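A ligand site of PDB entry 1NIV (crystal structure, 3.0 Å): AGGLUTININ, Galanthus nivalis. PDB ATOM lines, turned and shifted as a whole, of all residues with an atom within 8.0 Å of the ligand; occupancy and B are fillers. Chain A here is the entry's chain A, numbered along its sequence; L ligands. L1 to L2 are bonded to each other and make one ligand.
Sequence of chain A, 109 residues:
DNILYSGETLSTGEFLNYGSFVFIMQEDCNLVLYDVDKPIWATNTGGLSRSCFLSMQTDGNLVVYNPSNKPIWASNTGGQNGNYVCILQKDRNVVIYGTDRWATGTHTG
NE2 of Gln 57 is in hydrogen-bond range of O2 of LIG L1, at 2.6 Å.
ND2 of Asn 61 sits at hydrogen-bond distance from O5 of LIG L1, 2.8 Å away.
OH of Tyr 65 is in hydrogen-bond range of O4 of LIG L1 (2.8 Å).
O2 of LIG L1 sits at hydrogen-bond distance from OD2 of Asp 59, at 2.9 Å.
OH of Tyr 65 lies within hydrogen-bond range of OE1 of Gln 57 (2.4 Å).
NE2 of Gln 57 sits at hydrogen-bond distance from OD1 of Asp 59 (2.9 Å).
The side-chain carboxylate (OD1) of Asp 59 is in hydrogen-bond range of the backbone NH (N) of Asn 61 (3.0 Å).
N of Asn 76 lies within hydrogen-bond range of OD1 of Asn 61 (3.0 Å).
The backbone NH (N) of Ser 75 is in hydrogen-bond range of the side-chain amide oxygen (OD1) of Asn 61 (3.5 Å).
The backbone carbonyl oxygen of Asp 59 sits at hydrogen-bond distance from the backbone NH of Gly 79 (2.9 Å).
The backbone carbonyl oxygen (O) of Val 63 sits at hydrogen-bond distance from the backbone NH (N) of Ser 55 (2.7 Å).
Residues that only touch the ligand: Asn 76, Ala 74 and Val 63.
Hydrophobic or aromatic side chains that line the ligand: Val 63, Tyr 65 and Ala 74.
Seven residues have an atom within 4 Å of the ligand: Gln 57, Asp 59, Asn 61, Val 63, Tyr 65, Ala 74 and Asn 76.
The nearest printed residue that does not touch the ligand is Pro 71 (4.2 Å).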
ATOM      1  N   SER A  55     -23.474   3.688  11.825  1.00  0.00           N
ATOM      2  CA  SER A  55     -22.127   4.218  11.830  1.00  0.00           C
ATOM      3  C   SER A  55     -21.156   3.282  12.539  1.00  0.00           C
ATOM      4  O   SER A  55     -21.414   2.842  13.656  1.00  0.00           O
ATOM      5  CB  SER A  55     -22.146   5.570  12.525  1.00  0.00           C
ATOM      6  OG  SER A  55     -20.868   6.167  12.504  1.00  0.00           O
ATOM      7  N   MET A  56     -20.050   2.936  11.872  1.00  0.00           N
ATOM      8  CA  MET A  56     -19.018   2.096  12.476  1.00  0.00           C
ATOM      9  C   MET A  56     -17.991   3.093  12.975  1.00  0.00           C
ATOM     10  O   MET A  56     -17.307   3.723  12.173  1.00  0.00           O
ATOM     11  CB  MET A  56     -18.372   1.183  11.426  1.00  0.00           C
ATOM     12  CG  MET A  56     -17.157   0.404  11.906  1.00  0.00           C
ATOM     13  SD  MET A  56     -17.481  -0.965  13.026  1.00  0.00           S
ATOM     14  CE  MET A  56     -17.172  -0.232  14.627  1.00  0.00           C
ATOM     15  N   GLN A  57     -17.931   3.273  14.291  1.00  0.00           N
ATOM     16  CA  GLN A  57     -17.016   4.245  14.885  1.00  0.00           C
ATOM     17  C   GLN A  57     -15.590   3.733  15.100  1.00  0.00           C
ATOM     18  O   GLN A  57     -15.367   2.525  15.210  1.00  0.00           O
ATOM     19  CB  GLN A  57     -17.581   4.723  16.199  1.00  0.00           C
ATOM     20  CG  GLN A  57     -19.035   5.121  16.137  1.00  0.00           C
ATOM     21  CD  GLN A  57     -19.500   5.758  17.433  1.00  0.00           C
ATOM     22  OE1 GLN A  57     -20.293   6.678  17.412  1.00  0.00           O
ATOM     23  NE2 GLN A  57     -18.975   5.272  18.557  1.00  0.00           N
ATOM     24  N   THR A  58     -14.648   4.678  15.214  1.00  0.00           N
ATOM     25  CA  THR A  58     -13.227   4.369  15.426  1.00  0.00           C
ATOM     26  C   THR A  58     -12.947   3.849  16.824  1.00  0.00           C
ATOM     27  O   THR A  58     -11.903   3.258  17.068  1.00  0.00           O
ATOM     28  CB  THR A  58     -12.355   5.586  15.222  1.00  0.00           C
ATOM     29  OG1 THR A  58     -13.057   6.737  15.685  1.00  0.00           O
ATOM     30  CG2 THR A  58     -11.998   5.744  13.763  1.00  0.00           C
ATOM     31  N   ASP A  59     -13.837   4.153  17.752  1.00  0.00           N
ATOM     32  CA  ASP A  59     -13.678   3.660  19.096  1.00  0.00           C
ATOM     33  C   ASP A  59     -14.119   2.201  19.176  1.00  0.00           C
ATOM     34  O   ASP A  59     -13.963   1.568  20.218  1.00  0.00           O
ATOM     35  CB  ASP A  59     -14.453   4.539  20.086  1.00  0.00           C
ATOM     36  CG  ASP A  59     -15.953   4.421  19.932  1.00  0.00           C
ATOM     37  OD1 ASP A  59     -16.449   3.929  18.902  1.00  0.00           O
ATOM     38  OD2 ASP A  59     -16.640   4.844  20.875  1.00  0.00           O
ATOM     39  N   GLY A  60     -14.708   1.699  18.102  1.00  0.00           N
ATOM     40  CA  GLY A  60     -15.126   0.312  18.061  1.00  0.00           C
ATOM     41  C   GLY A  60     -16.600   0.075  18.277  1.00  0.00           C
ATOM     42  O   GLY A  60     -17.082  -1.054  18.175  1.00  0.00           O
ATOM     43  N   ASN A  61     -17.341   1.128  18.570  1.00  0.00           N
ATOM     44  CA  ASN A  61     -18.773   1.010  18.801  1.00  0.00           C
ATOM     45  C   ASN A  61     -19.551   1.051  17.480  1.00  0.00           C
ATOM     46  O   ASN A  61     -19.303   1.900  16.624  1.00  0.00           O
ATOM     47  CB  ASN A  61     -19.229   2.147  19.716  1.00  0.00           C
ATOM     48  CG  ASN A  61     -20.505   1.829  20.438  1.00  0.00           C
ATOM     49  OD1 ASN A  61     -21.194   0.864  20.117  1.00  0.00           O
ATOM     50  ND2 ASN A  61     -20.814   2.617  21.448  1.00  0.00           N
ATOM     51  N   LEU A  62     -20.466   0.107  17.299  1.00  0.00           N
ATOM     52  CA  LEU A  62     -21.270   0.070  16.087  1.00  0.00           C
ATOM     53  C   LEU A  62     -22.595   0.710  16.497  1.00  0.00           C
ATOM     54  O   LEU A  62     -23.411   0.073  17.157  1.00  0.00           O
ATOM     55  CB  LEU A  62     -21.483  -1.362  15.609  1.00  0.00           C
ATOM     56  CG  LEU A  62     -22.321  -1.478  14.326  1.00  0.00           C
ATOM     57  CD1 LEU A  62     -21.621  -0.791  13.171  1.00  0.00           C
ATOM     58  CD2 LEU A  62     -22.571  -2.926  13.995  1.00  0.00           C
ATOM     59  N   VAL A  63     -22.812   1.958  16.113  1.00  0.00           N
ATOM     60  CA  VAL A  63     -24.011   2.682  16.501  1.00  0.00           C
ATOM     61  C   VAL A  63     -24.993   3.044  15.398  1.00  0.00           C
ATOM     62  O   VAL A  63     -24.593   3.424  14.302  1.00  0.00           O
ATOM     63  CB  VAL A  63     -23.633   3.972  17.234  1.00  0.00           C
ATOM     64  CG1 VAL A  63     -24.869   4.714  17.668  1.00  0.00           C
ATOM     65  CG2 VAL A  63     -22.740   3.672  18.421  1.00  0.00           C
ATOM     66  N   VAL A  64     -26.287   2.972  15.714  1.00  0.00           N
ATOM     67  CA  VAL A  64     -27.357   3.370  14.800  1.00  0.00           C
ATOM     68  C   VAL A  64     -27.880   4.686  15.363  1.00  0.00           C
ATOM     69  O   VAL A  64     -28.410   4.723  16.474  1.00  0.00           O
ATOM     70  CB  VAL A  64     -28.498   2.329  14.793  1.00  0.00           C
ATOM     71  CG1 VAL A  64     -29.854   2.977  14.507  1.00  0.00           C
ATOM     72  CG2 VAL A  64     -28.201   1.253  13.761  1.00  0.00           C
ATOM     73  N   TYR A  65     -27.637   5.775  14.643  1.00  0.00           N
ATOM     74  CA  TYR A  65     -28.069   7.106  15.082  1.00  0.00           C
ATOM     75  C   TYR A  65     -29.282   7.592  14.342  1.00  0.00           C
ATOM     76  O   TYR A  65     -29.497   7.196  13.195  1.00  0.00           O
ATOM     77  CB  TYR A  65     -26.972   8.138  14.817  1.00  0.00           C
ATOM     78  CG  TYR A  65     -25.760   8.025  15.673  1.00  0.00           C
ATOM     79  CD1 TYR A  65     -25.761   8.512  16.969  1.00  0.00           C
ATOM     80  CD2 TYR A  65     -24.587   7.471  15.165  1.00  0.00           C
ATOM     81  CE1 TYR A  65     -24.624   8.461  17.754  1.00  0.00           C
ATOM     82  CE2 TYR A  65     -23.429   7.408  15.948  1.00  0.00           C
ATOM     83  CZ  TYR A  65     -23.456   7.901  17.234  1.00  0.00           C
ATOM     84  OH  TYR A  65     -22.327   7.866  18.005  1.00  0.00           O
ATOM     85  N   ASN A  69     -29.135  12.700  15.792  1.00  0.00           N
ATOM     86  CA  ASN A  69     -27.908  12.162  16.369  1.00  0.00           C
ATOM     87  C   ASN A  69     -28.027  11.466  17.711  1.00  0.00           C
ATOM     88  O   ASN A  69     -27.022  11.221  18.376  1.00  0.00           O
ATOM     89  CB  ASN A  69     -26.804  13.211  16.395  1.00  0.00           C
ATOM     90  CG  ASN A  69     -25.918  13.117  15.192  1.00  0.00           C
ATOM     91  OD1 ASN A  69     -24.719  12.874  15.317  1.00  0.00           O
ATOM     92  ND2 ASN A  69     -26.506  13.256  14.012  1.00  0.00           N
ATOM     93  N   LYS A  70     -29.241  11.142  18.128  1.00  0.00           N
ATOM     94  CA  LYS A  70     -29.432  10.433  19.369  1.00  0.00           C
ATOM     95  C   LYS A  70     -29.234   8.997  18.945  1.00  0.00           C
ATOM     96  O   LYS A  70     -29.702   8.584  17.864  1.00  0.00           O
ATOM     97  CB  LYS A  70     -30.846  10.620  19.912  1.00  0.00           C
ATOM     98  CG  LYS A  70     -31.049   9.948  21.263  1.00  0.00           C
ATOM     99  CD  LYS A  70     -32.453   9.415  21.465  1.00  0.00           C
ATOM    100  CE  LYS A  70     -32.480   8.431  22.637  1.00  0.00           C
ATOM    101  NZ  LYS A  70     -33.810   7.818  22.904  1.00  0.00           N
ATOM    102  N   PRO A  71     -28.443   8.231  19.690  1.00  0.00           N
ATOM    103  CA  PRO A  71     -28.198   6.832  19.364  1.00  0.00           C
ATOM    104  C   PRO A  71     -29.423   5.999  19.722  1.00  0.00           C
ATOM    105  O   PRO A  71     -29.921   6.094  20.842  1.00  0.00           O
ATOM    106  CB  PRO A  71     -27.008   6.473  20.230  1.00  0.00           C
ATOM    107  CG  PRO A  71     -27.161   7.343  21.400  1.00  0.00           C
ATOM    108  CD  PRO A  71     -27.565   8.668  20.801  1.00  0.00           C
ATOM    109  N   ILE A  72     -29.957   5.269  18.747  1.00  0.00           N
ATOM    110  CA  ILE A  72     -31.115   4.413  18.942  1.00  0.00           C
ATOM    111  C   ILE A  72     -30.677   3.007  19.369  1.00  0.00           C
ATOM    112  O   ILE A  72     -31.377   2.321  20.122  1.00  0.00           O
ATOM    113  CB  ILE A  72     -31.896   4.279  17.639  1.00  0.00           C
ATOM    114  CG1 ILE A  72     -32.320   5.659  17.161  1.00  0.00           C
ATOM    115  CG2 ILE A  72     -33.094   3.372  17.808  1.00  0.00           C
ATOM    116  CD1 ILE A  72     -33.050   6.486  18.204  1.00  0.00           C
ATOM    117  N   TRP A  73     -29.527   2.566  18.878  1.00  0.00           N
ATOM    118  CA  TRP A  73     -29.007   1.242  19.174  1.00  0.00           C
ATOM    119  C   TRP A  73     -27.492   1.321  19.009  1.00  0.00           C
ATOM    120  O   TRP A  73     -26.993   2.207  18.301  1.00  0.00           O
ATOM    121  CB  TRP A  73     -29.583   0.225  18.179  1.00  0.00           C
ATOM    122  CG  TRP A  73     -29.050  -1.160  18.309  1.00  0.00           C
ATOM    123  CD1 TRP A  73     -29.566  -2.145  19.091  1.00  0.00           C
ATOM    124  CD2 TRP A  73     -27.879  -1.706  17.689  1.00  0.00           C
ATOM    125  NE1 TRP A  73     -28.781  -3.281  19.001  1.00  0.00           N
ATOM    126  CE2 TRP A  73     -27.746  -3.038  18.147  1.00  0.00           C
ATOM    127  CE3 TRP A  73     -26.936  -1.208  16.786  1.00  0.00           C
ATOM    128  CZ2 TRP A  73     -26.687  -3.883  17.739  1.00  0.00           C
ATOM    129  CZ3 TRP A  73     -25.876  -2.043  16.381  1.00  0.00           C
ATOM    130  CH2 TRP A  73     -25.776  -3.371  16.866  1.00  0.00           C
ATOM    131  N   ALA A  74     -26.780   0.389  19.635  1.00  0.00           N
ATOM    132  CA  ALA A  74     -25.318   0.345  19.561  1.00  0.00           C
ATOM    133  C   ALA A  74     -24.830  -0.998  20.071  1.00  0.00           C
ATOM    134  O   ALA A  74     -25.492  -1.618  20.901  1.00  0.00           O
ATOM    135  CB  ALA A  74     -24.718   1.460  20.388  1.00  0.00           C
ATOM    136  N   SER A  75     -23.699  -1.461  19.556  1.00  0.00           N
ATOM    137  CA  SER A  75     -23.178  -2.739  19.995  1.00  0.00           C
ATOM    138  C   SER A  75     -22.521  -2.589  21.369  1.00  0.00           C
ATOM    139  O   SER A  75     -22.245  -3.575  22.056  1.00  0.00           O
ATOM    140  CB  SER A  75     -22.184  -3.299  18.986  1.00  0.00           C
ATOM    141  OG  SER A  75     -21.238  -2.310  18.632  1.00  0.00           O
ATOM    142  N   ASN A  76     -22.258  -1.351  21.753  1.00  0.00           N
ATOM    143  CA  ASN A  76     -21.627  -1.050  23.033  1.00  0.00           C
ATOM    144  C   ASN A  76     -20.197  -1.542  23.128  1.00  0.00           C
ATOM    145  O   ASN A  76     -19.660  -1.664  24.209  1.00  0.00           O
ATOM    146  CB  ASN A  76     -22.447  -1.619  24.180  1.00  0.00           C
ATOM    147  CG  ASN A  76     -23.737  -0.876  24.372  1.00  0.00           C
ATOM    148  OD1 ASN A  76     -23.867   0.289  24.000  1.00  0.00           O
ATOM    149  ND2 ASN A  76     -24.705  -1.553  24.967  1.00  0.00           N
ATOM    150  N   THR A  77     -19.588  -1.827  21.982  1.00  0.00           N
ATOM    151  CA  THR A  77     -18.214  -2.279  21.943  1.00  0.00           C
ATOM    152  C   THR A  77     -17.266  -1.085  21.790  1.00  0.00           C
ATOM    153  O   THR A  77     -16.221  -1.191  21.147  1.00  0.00           O
ATOM    154  CB  THR A  77     -18.017  -3.222  20.762  1.00  0.00           C
ATOM    155  OG1 THR A  77     -18.684  -2.687  19.613  1.00  0.00           O
ATOM    156  CG2 THR A  77     -18.574  -4.606  21.079  1.00  0.00           C
ATOM    157  N   GLY A  78     -17.667   0.071  22.334  1.00  0.00           N
ATOM    158  CA  GLY A  78     -16.853   1.271  22.252  1.00  0.00           C
ATOM    159  C   GLY A  78     -15.759   1.263  23.289  1.00  0.00           C
ATOM    160  O   GLY A  78     -15.898   0.654  24.350  1.00  0.00           O
ATOM    161  N   GLY A  79     -14.635   1.911  22.997  1.00  0.00           N
ATOM    162  CA  GLY A  79     -13.562   1.929  23.960  1.00  0.00           C
ATOM    163  C   GLY A  79     -12.185   2.216  23.403  1.00  0.00           C
ATOM    164  O   GLY A  79     -11.660   3.308  23.633  1.00  0.00           O
ATOM    165  N   ASN A  81      -9.667   3.359  20.797  1.00  0.00           N
ATOM    166  CA  ASN A  81      -9.625   4.126  19.572  1.00  0.00           C
ATOM    167  C   ASN A  81      -8.702   3.400  18.600  1.00  0.00           C
ATOM    168  O   ASN A  81      -7.611   2.979  18.991  1.00  0.00           O
ATOM    169  CB  ASN A  81      -9.119   5.527  19.834  1.00  0.00           C
ATOM    170  CG  ASN A  81      -9.113   6.379  18.587  1.00  0.00           C
ATOM    171  OD1 ASN A  81     -10.111   7.019  18.249  1.00  0.00           O
ATOM    172  ND2 ASN A  81      -8.007   6.358  17.868  1.00  0.00           N
HETATM  173  C1  LIG L   1     -20.248   5.562  23.339  1.00  0.00           C
HETATM  174  C2  LIG L   1     -19.638   6.177  22.104  1.00  0.00           C
HETATM  175  C3  LIG L   1     -20.610   7.180  21.569  1.00  0.00           C
HETATM  176  C4  LIG L   1     -21.876   6.454  21.192  1.00  0.00           C
HETATM  177  C5  LIG L   1     -22.444   5.729  22.403  1.00  0.00           C
HETATM  178  C6  LIG L   1     -23.625   4.841  22.079  1.00  0.00           C
HETATM  179  C7  LIG L   1     -21.166   6.159  25.490  1.00  0.00           C
HETATM  180  O1  LIG L   1     -20.567   6.565  24.249  1.00  0.00           O
HETATM  181  O2  LIG L   1     -19.460   5.172  21.137  1.00  0.00           O
HETATM  182  O3  LIG L   1     -20.052   7.768  20.391  1.00  0.00           O
HETATM  183  O4  LIG L   1     -22.818   7.381  20.720  1.00  0.00           O
HETATM  184  O5  LIG L   1     -21.444   4.868  22.979  1.00  0.00           O
HETATM  185  O6  LIG L   1     -23.837   3.906  23.119  1.00  0.00           O
HETATM  186  C1  LG2 L   2     -19.807   9.139  20.454  1.00  0.00           C
HETATM  187  C2  LG2 L   2     -19.622   9.657  19.030  1.00  0.00           C
HETATM  188  C3  LG2 L   2     -18.316   9.137  18.431  1.00  0.00           C
HETATM  189  C4  LG2 L   2     -17.152   9.472  19.348  1.00  0.00           C
HETATM  190  C5  LG2 L   2     -17.424   8.909  20.735  1.00  0.00           C
HETATM  191  C6  LG2 L   2     -16.354   9.300  21.725  1.00  0.00           C
HETATM  192  O1  LG2 L   2     -19.619  11.067  19.060  1.00  0.00           O
HETATM  193  O2  LG2 L   2     -18.108   9.718  17.158  1.00  0.00           O
HETATM  194  O3  LG2 L   2     -15.943   8.921  18.825  1.00  0.00           O
HETATM  195  O4  LG2 L   2     -18.664   9.459  21.236  1.00  0.00           O
HETATM  196  O5  LG2 L   2     -16.466  10.678  22.056  1.00  0.00           O
